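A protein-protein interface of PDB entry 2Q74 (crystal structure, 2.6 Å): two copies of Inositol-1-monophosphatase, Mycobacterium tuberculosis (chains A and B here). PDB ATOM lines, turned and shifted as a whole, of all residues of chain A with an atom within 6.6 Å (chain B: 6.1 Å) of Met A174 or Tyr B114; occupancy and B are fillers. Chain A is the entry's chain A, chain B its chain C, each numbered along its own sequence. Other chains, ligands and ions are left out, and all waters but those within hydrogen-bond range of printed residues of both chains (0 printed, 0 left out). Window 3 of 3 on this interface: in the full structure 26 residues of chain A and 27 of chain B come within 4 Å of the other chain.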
ATOM      1  N   THR A 167      -5.960  14.492  37.149  1.00  0.00           N
ATOM      2  CA  THR A 167      -5.731  15.229  35.928  1.00  0.00           C
ATOM      3  C   THR A 167      -6.295  16.634  36.047  1.00  0.00           C
ATOM      4  O   THR A 167      -6.968  16.948  37.011  1.00  0.00           O
ATOM      5  CB  THR A 167      -6.394  14.514  34.741  1.00  0.00           C
ATOM      6  OG1 THR A 167      -7.807  14.502  34.940  1.00  0.00           O
ATOM      7  CG2 THR A 167      -5.906  13.092  34.618  1.00  0.00           C
ATOM      8  N   VAL A 169      -8.374  18.038  33.518  1.00  0.00           N
ATOM      9  CA  VAL A 169      -9.431  18.175  32.507  1.00  0.00           C
ATOM     10  C   VAL A 169     -10.440  19.245  32.878  1.00  0.00           C
ATOM     11  O   VAL A 169     -10.818  19.338  34.044  1.00  0.00           O
ATOM     12  CB  VAL A 169     -10.295  16.874  32.323  1.00  0.00           C
ATOM     13  CG1 VAL A 169     -10.140  16.313  30.928  1.00  0.00           C
ATOM     14  CG2 VAL A 169     -10.049  15.864  33.444  1.00  0.00           C
ATOM     15  N   ASP A 170     -10.909  19.985  31.869  1.00  0.00           N
ATOM     16  CA  ASP A 170     -11.946  21.047  32.034  1.00  0.00           C
ATOM     17  C   ASP A 170     -13.272  20.648  31.411  1.00  0.00           C
ATOM     18  O   ASP A 170     -14.322  20.880  32.000  1.00  0.00           O
ATOM     19  CB  ASP A 170     -11.507  22.346  31.367  1.00  0.00           C
ATOM     20  CG  ASP A 170     -10.253  22.887  31.961  1.00  0.00           C
ATOM     21  OD1 ASP A 170      -9.973  22.550  33.133  1.00  0.00           O
ATOM     22  OD2 ASP A 170      -9.538  23.634  31.249  1.00  0.00           O
ATOM     23  N   GLU A 171     -13.221  20.082  30.207  1.00  0.00           N
ATOM     24  CA  GLU A 171     -14.424  19.730  29.497  1.00  0.00           C
ATOM     25  C   GLU A 171     -14.792  18.284  29.781  1.00  0.00           C
ATOM     26  O   GLU A 171     -14.027  17.366  29.482  1.00  0.00           O
ATOM     27  CB  GLU A 171     -14.258  19.954  27.988  1.00  0.00           C
ATOM     28  CG  GLU A 171     -14.076  21.420  27.578  1.00  0.00           C
ATOM     29  CD  GLU A 171     -12.709  21.697  26.959  1.00  0.00           C
ATOM     30  OE1 GLU A 171     -11.685  21.658  27.687  1.00  0.00           O
ATOM     31  OE2 GLU A 171     -12.663  21.952  25.735  1.00  0.00           O
ATOM     32  N   LEU A 172     -15.979  18.093  30.342  1.00  0.00           N
ATOM     33  CA  LEU A 172     -16.517  16.761  30.594  1.00  0.00           C
ATOM     34  C   LEU A 172     -16.541  15.883  29.355  1.00  0.00           C
ATOM     35  O   LEU A 172     -16.528  14.697  29.493  1.00  0.00           O
ATOM     36  CB  LEU A 172     -17.933  16.854  31.185  1.00  0.00           C
ATOM     37  CG  LEU A 172     -18.586  15.558  31.694  1.00  0.00           C
ATOM     38  CD1 LEU A 172     -17.797  14.940  32.870  1.00  0.00           C
ATOM     39  CD2 LEU A 172     -20.059  15.847  32.077  1.00  0.00           C
ATOM     40  N   SER A 173     -16.576  16.465  28.159  1.00  0.00           N
ATOM     41  CA  SER A 173     -16.502  15.699  26.898  1.00  0.00           C
ATOM     42  C   SER A 173     -15.109  15.190  26.622  1.00  0.00           C
ATOM     43  O   SER A 173     -14.895  14.442  25.675  1.00  0.00           O
ATOM     44  CB  SER A 173     -16.911  16.570  25.715  1.00  0.00           C
ATOM     45  OG  SER A 173     -15.977  17.611  25.528  1.00  0.00           O
ATOM     46  N   MET A 174     -14.163  15.622  27.446  1.00  0.00           N
ATOM     47  CA  MET A 174     -12.777  15.203  27.354  1.00  0.00           C
ATOM     48  C   MET A 174     -12.401  14.225  28.475  1.00  0.00           C
ATOM     49  O   MET A 174     -11.254  13.795  28.570  1.00  0.00           O
ATOM     50  CB  MET A 174     -11.893  16.444  27.442  1.00  0.00           C
ATOM     51  CG  MET A 174     -11.971  17.326  26.218  1.00  0.00           C
ATOM     52  SD  MET A 174     -10.960  16.656  24.876  1.00  0.00           S
ATOM     53  CE  MET A 174     -12.063  15.515  23.989  1.00  0.00           C
ATOM     54  N   ALA A 175     -13.372  13.881  29.318  1.00  0.00           N
ATOM     55  CA  ALA A 175     -13.109  13.106  30.512  1.00  0.00           C
ATOM     56  C   ALA A 175     -13.296  11.602  30.250  1.00  0.00           C
ATOM     57  O   ALA A 175     -14.237  11.195  29.566  1.00  0.00           O
ATOM     58  CB  ALA A 175     -14.003  13.577  31.629  1.00  0.00           C
ATOM     59  N   LEU A 176     -12.377  10.794  30.784  1.00  0.00           N
ATOM     60  CA  LEU A 176     -12.519   9.345  30.758  1.00  0.00           C
ATOM     61  C   LEU A 176     -13.151   8.891  32.076  1.00  0.00           C
ATOM     62  O   LEU A 176     -12.573   9.075  33.162  1.00  0.00           O
ATOM     63  CB  LEU A 176     -11.155   8.692  30.561  1.00  0.00           C
ATOM     64  CG  LEU A 176     -11.052   7.203  30.432  1.00  0.00           C
ATOM     65  CD1 LEU A 176     -11.795   6.734  29.205  1.00  0.00           C
ATOM     66  CD2 LEU A 176      -9.577   6.870  30.354  1.00  0.00           C
ATOM     67  N   LEU A 201     -21.832  12.548  26.674  1.00  0.00           N
ATOM     68  CA  LEU A 201     -21.293  13.763  27.280  1.00  0.00           C
ATOM     69  C   LEU A 201     -19.829  13.626  27.668  1.00  0.00           C
ATOM     70  O   LEU A 201     -19.243  14.613  28.138  1.00  0.00           O
ATOM     71  CB  LEU A 201     -22.070  14.116  28.539  1.00  0.00           C
ATOM     72  CG  LEU A 201     -23.542  14.443  28.343  1.00  0.00           C
ATOM     73  CD1 LEU A 201     -24.192  14.573  29.701  1.00  0.00           C
ATOM     74  CD2 LEU A 201     -23.704  15.716  27.536  1.00  0.00           C
ATOM     75  N   VAL A 202     -19.256  12.420  27.512  1.00  0.00           N
ATOM     76  CA  VAL A 202     -17.878  12.154  27.946  1.00  0.00           C
ATOM     77  C   VAL A 202     -17.029  11.502  26.873  1.00  0.00           C
ATOM     78  O   VAL A 202     -17.539  10.864  25.953  1.00  0.00           O
ATOM     79  CB  VAL A 202     -17.818  11.250  29.205  1.00  0.00           C
ATOM     80  CG1 VAL A 202     -18.427  11.955  30.416  1.00  0.00           C
ATOM     81  CG2 VAL A 202     -18.475   9.876  28.939  1.00  0.00           C
ATOM     82  N   ARG A 203     -15.717  11.663  27.027  1.00  0.00           N
ATOM     83  CA  ARG A 203     -14.724  11.125  26.095  1.00  0.00           C
ATOM     84  C   ARG A 203     -14.931   9.658  25.808  1.00  0.00           C
ATOM     85  O   ARG A 203     -15.082   9.298  24.655  1.00  0.00           O
ATOM     86  CB  ARG A 203     -13.348  11.322  26.690  1.00  0.00           C
ATOM     87  CG  ARG A 203     -12.163  11.012  25.810  1.00  0.00           C
ATOM     88  CD  ARG A 203     -10.917  11.239  26.682  1.00  0.00           C
ATOM     89  NE  ARG A 203      -9.672  11.170  25.949  1.00  0.00           N
ATOM     90  CZ  ARG A 203      -9.165  12.151  25.221  1.00  0.00           C
ATOM     91  NH1 ARG A 203      -9.806  13.303  25.076  1.00  0.00           N
ATOM     92  NH2 ARG A 203      -8.011  11.944  24.593  1.00  0.00           N
ATOM     93  N   ASP A 204     -14.911   8.816  26.846  1.00  0.00           N
ATOM     94  CA  ASP A 204     -15.132   7.359  26.735  1.00  0.00           C
ATOM     95  C   ASP A 204     -15.443   6.814  28.142  1.00  0.00           C
ATOM     96  O   ASP A 204     -15.402   7.538  29.131  1.00  0.00           O
ATOM     97  CB  ASP A 204     -13.913   6.649  26.133  1.00  0.00           C
ATOM     98  CG  ASP A 204     -14.268   5.286  25.449  1.00  0.00           C
ATOM     99  OD1 ASP A 204     -15.374   4.756  25.663  1.00  0.00           O
ATOM    100  OD2 ASP A 204     -13.424   4.718  24.700  1.00  0.00           O
ATOM    101  N   ALA A 220      -4.437   8.586  40.444  1.00  0.00           N
ATOM    102  CA  ALA A 220      -3.219   8.502  39.651  1.00  0.00           C
ATOM    103  C   ALA A 220      -3.324   9.259  38.335  1.00  0.00           C
ATOM    104  O   ALA A 220      -2.312   9.550  37.717  1.00  0.00           O
ATOM    105  CB  ALA A 220      -2.899   7.079  39.369  1.00  0.00           C
ATOM    106  N   GLY A 221      -4.540   9.577  37.899  1.00  0.00           N
ATOM    107  CA  GLY A 221      -4.758  10.245  36.608  1.00  0.00           C
ATOM    108  C   GLY A 221      -5.033   9.264  35.480  1.00  0.00           C
ATOM    109  O   GLY A 221      -4.984   9.638  34.323  1.00  0.00           O
ATOM    110  N   ARG A 222      -5.330   8.015  35.804  1.00  0.00           N
ATOM    111  CA  ARG A 222      -5.661   7.027  34.770  1.00  0.00           C
ATOM    112  C   ARG A 222      -7.134   7.060  34.366  1.00  0.00           C
ATOM    113  O   ARG A 222      -7.496   6.536  33.328  1.00  0.00           O
ATOM    114  CB  ARG A 222      -5.283   5.641  35.249  1.00  0.00           C
ATOM    115  CG  ARG A 222      -3.844   5.580  35.656  1.00  0.00           C
ATOM    116  CD  ARG A 222      -3.357   4.166  35.781  1.00  0.00           C
ATOM    117  NE  ARG A 222      -2.103   4.117  36.519  1.00  0.00           N
ATOM    118  CZ  ARG A 222      -1.348   3.032  36.663  1.00  0.00           C
ATOM    119  NH1 ARG A 222      -1.699   1.874  36.105  1.00  0.00           N
ATOM    120  NH2 ARG A 222      -0.224   3.117  37.374  1.00  0.00           N
ATOM    121  N   LEU A 223      -7.967   7.654  35.211  1.00  0.00           N
ATOM    122  CA  LEU A 223      -9.325   8.037  34.860  1.00  0.00           C
ATOM    123  C   LEU A 223      -9.473   9.494  35.269  1.00  0.00           C
ATOM    124  O   LEU A 223      -8.808   9.932  36.207  1.00  0.00           O
ATOM    125  CB  LEU A 223     -10.349   7.216  35.635  1.00  0.00           C
ATOM    126  CG  LEU A 223     -10.402   5.715  35.371  1.00  0.00           C
ATOM    127  CD1 LEU A 223     -11.373   5.136  36.396  1.00  0.00           C
ATOM    128  CD2 LEU A 223     -10.807   5.369  33.918  1.00  0.00           C
ATOM    129  N   ASP A 224     -10.354  10.229  34.584  1.00  0.00           N
ATOM    130  CA  ASP A 224     -10.671  11.600  34.946  1.00  0.00           C
ATOM    131  C   ASP A 224     -11.778  11.651  35.988  1.00  0.00           C
ATOM    132  O   ASP A 224     -11.887  12.629  36.732  1.00  0.00           O
ATOM    133  CB  ASP A 224     -11.102  12.383  33.718  1.00  0.00           C
ATOM    134  CG  ASP A 224      -9.956  12.650  32.754  1.00  0.00           C
ATOM    135  OD1 ASP A 224      -8.859  13.095  33.149  1.00  0.00           O
ATOM    136  OD2 ASP A 224     -10.169  12.392  31.561  1.00  0.00           O
ATOM    137  N   ILE A 271     -13.822  19.340  36.529  1.00  0.00           N
ATOM    138  CA  ILE A 271     -14.905  18.680  35.816  1.00  0.00           C
ATOM    139  C   ILE A 271     -16.006  18.125  36.728  1.00  0.00           C
ATOM    140  O   ILE A 271     -17.013  17.608  36.258  1.00  0.00           O
ATOM    141  CB  ILE A 271     -14.284  17.586  34.908  1.00  0.00           C
ATOM    142  CG1 ILE A 271     -14.795  17.754  33.482  1.00  0.00           C
ATOM    143  CG2 ILE A 271     -14.447  16.149  35.483  1.00  0.00           C
ATOM    144  CD1 ILE A 271     -13.767  17.295  32.460  1.00  0.00           C
ATOM    145  N   ARG B  30       7.225   4.850  24.604  1.00  0.00           N
ATOM    146  CA  ARG B  30       6.275   5.499  25.512  1.00  0.00           C
ATOM    147  C   ARG B  30       6.988   6.147  26.701  1.00  0.00           C
ATOM    148  O   ARG B  30       6.677   7.281  27.068  1.00  0.00           O
ATOM    149  CB  ARG B  30       5.205   4.522  26.016  1.00  0.00           C
ATOM    150  CG  ARG B  30       4.179   5.204  26.925  1.00  0.00           C
ATOM    151  CD  ARG B  30       3.024   4.292  27.418  1.00  0.00           C
ATOM    152  NE  ARG B  30       2.633   4.671  28.778  1.00  0.00           N
ATOM    153  CZ  ARG B  30       2.015   5.801  29.106  1.00  0.00           C
ATOM    154  NH1 ARG B  30       1.672   6.678  28.175  1.00  0.00           N
ATOM    155  NH2 ARG B  30       1.728   6.070  30.367  1.00  0.00           N
ATOM    156  N   THR B 109      -5.535   3.426  22.158  1.00  0.00           N
ATOM    157  CA  THR B 109      -4.768   4.668  22.186  1.00  0.00           C
ATOM    158  C   THR B 109      -5.160   5.572  23.350  1.00  0.00           C
ATOM    159  O   THR B 109      -4.326   6.336  23.843  1.00  0.00           O
ATOM    160  CB  THR B 109      -4.934   5.495  20.871  1.00  0.00           C
ATOM    161  OG1 THR B 109      -6.321   5.552  20.505  1.00  0.00           O
ATOM    162  CG2 THR B 109      -4.152   4.883  19.712  1.00  0.00           C
ATOM    163  N   VAL B 110      -6.424   5.501  23.772  1.00  0.00           N
ATOM    164  CA  VAL B 110      -6.868   6.219  24.956  1.00  0.00           C
ATOM    165  C   VAL B 110      -6.171   5.638  26.171  1.00  0.00           C
ATOM    166  O   VAL B 110      -5.674   6.388  27.028  1.00  0.00           O
ATOM    167  CB  VAL B 110      -8.389   6.162  25.135  1.00  0.00           C
ATOM    168  CG1 VAL B 110      -8.796   6.731  26.490  1.00  0.00           C
ATOM    169  CG2 VAL B 110      -9.061   6.946  24.028  1.00  0.00           C
ATOM    170  N   ASN B 111      -6.116   4.310  26.225  1.00  0.00           N
ATOM    171  CA  ASN B 111      -5.445   3.598  27.303  1.00  0.00           C
ATOM    172  C   ASN B 111      -3.976   3.970  27.376  1.00  0.00           C
ATOM    173  O   ASN B 111      -3.465   4.310  28.443  1.00  0.00           O
ATOM    174  CB  ASN B 111      -5.621   2.079  27.128  1.00  0.00           C
ATOM    175  CG  ASN B 111      -6.922   1.595  27.692  1.00  0.00           C
ATOM    176  OD1 ASN B 111      -7.493   2.291  28.515  1.00  0.00           O
ATOM    177  ND2 ASN B 111      -7.411   0.416  27.264  1.00  0.00           N
ATOM    178  N   PHE B 112      -3.319   3.901  26.220  1.00  0.00           N
ATOM    179  CA  PHE B 112      -1.919   4.295  26.066  1.00  0.00           C
ATOM    180  C   PHE B 112      -1.637   5.678  26.629  1.00  0.00           C
ATOM    181  O   PHE B 112      -0.671   5.856  27.347  1.00  0.00           O
ATOM    182  CB  PHE B 112      -1.534   4.271  24.590  1.00  0.00           C
ATOM    183  CG  PHE B 112      -0.098   4.627  24.320  1.00  0.00           C
ATOM    184  CD1 PHE B 112       0.875   3.652  24.323  1.00  0.00           C
ATOM    185  CD2 PHE B 112       0.264   5.928  24.028  1.00  0.00           C
ATOM    186  CE1 PHE B 112       2.189   3.965  24.059  1.00  0.00           C
ATOM    187  CE2 PHE B 112       1.574   6.257  23.767  1.00  0.00           C
ATOM    188  CZ  PHE B 112       2.542   5.274  23.783  1.00  0.00           C
ATOM    189  N   VAL B 113      -2.486   6.638  26.294  1.00  0.00           N
ATOM    190  CA  VAL B 113      -2.293   8.026  26.734  1.00  0.00           C
ATOM    191  C   VAL B 113      -2.465   8.180  28.249  1.00  0.00           C
ATOM    192  O   VAL B 113      -1.716   8.908  28.869  1.00  0.00           O
ATOM    193  CB  VAL B 113      -3.230   8.999  25.954  1.00  0.00           C
ATOM    194  CG1 VAL B 113      -3.291  10.372  26.599  1.00  0.00           C
ATOM    195  CG2 VAL B 113      -2.766   9.112  24.501  1.00  0.00           C
ATOM    196  N   TYR B 114      -3.415   7.462  28.834  1.00  0.00           N
ATOM    197  CA  TYR B 114      -3.706   7.565  30.273  1.00  0.00           C
ATOM    198  C   TYR B 114      -2.877   6.640  31.169  1.00  0.00           C
ATOM    199  O   TYR B 114      -2.876   6.786  32.387  1.00  0.00           O
ATOM    200  CB  TYR B 114      -5.183   7.264  30.540  1.00  0.00           C
ATOM    201  CG  TYR B 114      -6.133   8.420  30.315  1.00  0.00           C
ATOM    202  CD1 TYR B 114      -6.596   8.720  29.032  1.00  0.00           C
ATOM    203  CD2 TYR B 114      -6.610   9.176  31.384  1.00  0.00           C
ATOM    204  CE1 TYR B 114      -7.478   9.766  28.806  1.00  0.00           C
ATOM    205  CE2 TYR B 114      -7.512  10.247  31.180  1.00  0.00           C
ATOM    206  CZ  TYR B 114      -7.934  10.539  29.880  1.00  0.00           C
ATOM    207  OH  TYR B 114      -8.837  11.517  29.616  1.00  0.00           O
ATOM    208  N   GLY B 115      -2.194   5.673  30.578  1.00  0.00           N
ATOM    209  CA  GLY B 115      -1.383   4.754  31.353  1.00  0.00           C
ATOM    210  C   GLY B 115      -2.205   3.630  31.944  1.00  0.00           C
ATOM    211  O   GLY B 115      -1.847   3.066  32.965  1.00  0.00           O
ATOM    212  N   ILE B 116      -3.297   3.277  31.293  1.00  0.00           N
ATOM    213  CA  ILE B 116      -4.028   2.070  31.654  1.00  0.00           C
ATOM    214  C   ILE B 116      -3.406   0.903  30.858  1.00  0.00           C
ATOM    215  O   ILE B 116      -3.444   0.917  29.640  1.00  0.00           O
ATOM    216  CB  ILE B 116      -5.515   2.230  31.291  1.00  0.00           C
ATOM    217  CG1 ILE B 116      -6.115   3.427  32.036  1.00  0.00           C
ATOM    218  CG2 ILE B 116      -6.289   0.969  31.600  1.00  0.00           C
ATOM    219  CD1 ILE B 116      -7.605   3.700  31.701  1.00  0.00           C
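The side-chain carboxylate (OD1) of Asp A224 lies within hydrogen-bond range of the side-chain hydroxyl (OG1) of Thr A167 (2.5 Å). O of Ser A173 is in hydrogen-bond range of N of Arg A203 (3.2 Å). SD of Met A174 lies close to NH1 of Arg A203 (3.6 Å). O of Ala A175 sits at hydrogen-bond distance from N of Arg A203. The backbone NH (N) of Leu A176 is in hydrogen-bond range of the side-chain carboxylate (OD2) of Asp A224 (2.8 Å). The backbone NH (N) of Ile B116 sits at hydrogen-bond distance from the backbone carbonyl oxygen (O) of Asn B111 (3.0 Å).
No position is printed for both chains. Of the 10 pairs that touch across the chains among the printed residues, none has its exchanged pair printed and touching as well.
Leu A176 touches Val B110. Leu A176 touches Tyr B114 (CD2 to CD1, 3.7 Å). Ile B116 touches Leu A176 (CD1 to CD2, 3.97 Å). Tyr B114 touches Arg A203 (OH to CD, 3.6 Å). Gly A221 touches Tyr B114. Arg A222 touches Tyr B114. Arg A222 touches Ile B116.
Of the 9 printed residues of chain B, 4 touch a printed residue of chain A. Of the 19 printed residues of chain A, 6 touch a printed residue of chain B. Hydrophobic or aromatic side chains of chain A within 4 Å of the printed part of chain B: Leu A176.
Of chain B, only Tyr B114 comes within 4 Å of Met A174. Printed residues of chain A within 4 Å of Tyr B114: Met A174 (3.5 Å), Leu A176 (3.7 Å), Arg A203 (3.6 Å), Gly A221 (3.4 Å), Arg A222 (3.4 Å) and Asp A224 (2.5 Å). Printed residues of chain B within 4 Å of Arg A203: Tyr B114 (3.6 Å). Printed residues of chain B within 4 Å of Leu A176: Val B110 (3.9 Å), Tyr B114 (3.7 Å) and Ile B116 (3.97 Å). Printed residues of chain A within 4 Å of Gly B115: Arg A222 (3.4 Å). The nearest printed residue of chain B that does not touch Met A174 is Val B110 (7.8 Å). The nearest printed residue of chain B that does not touch Leu A176 is Asn B111 (5.4 Å).
The backbone carbonyl oxygen of Met A174 lies within hydrogen-bond range of the side-chain hydroxyl of Tyr B114 (3.5 Å). The backbone carbonyl oxygen (O) of Gly B115 lies within hydrogen-bond range of the guanidinium group (NH1) of Arg A222, 3.4 Å away. The side-chain hydroxyl of Tyr B114 lies within hydrogen-bond range of the side-chain carboxylate of Asp A224, at 2.5 Å.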
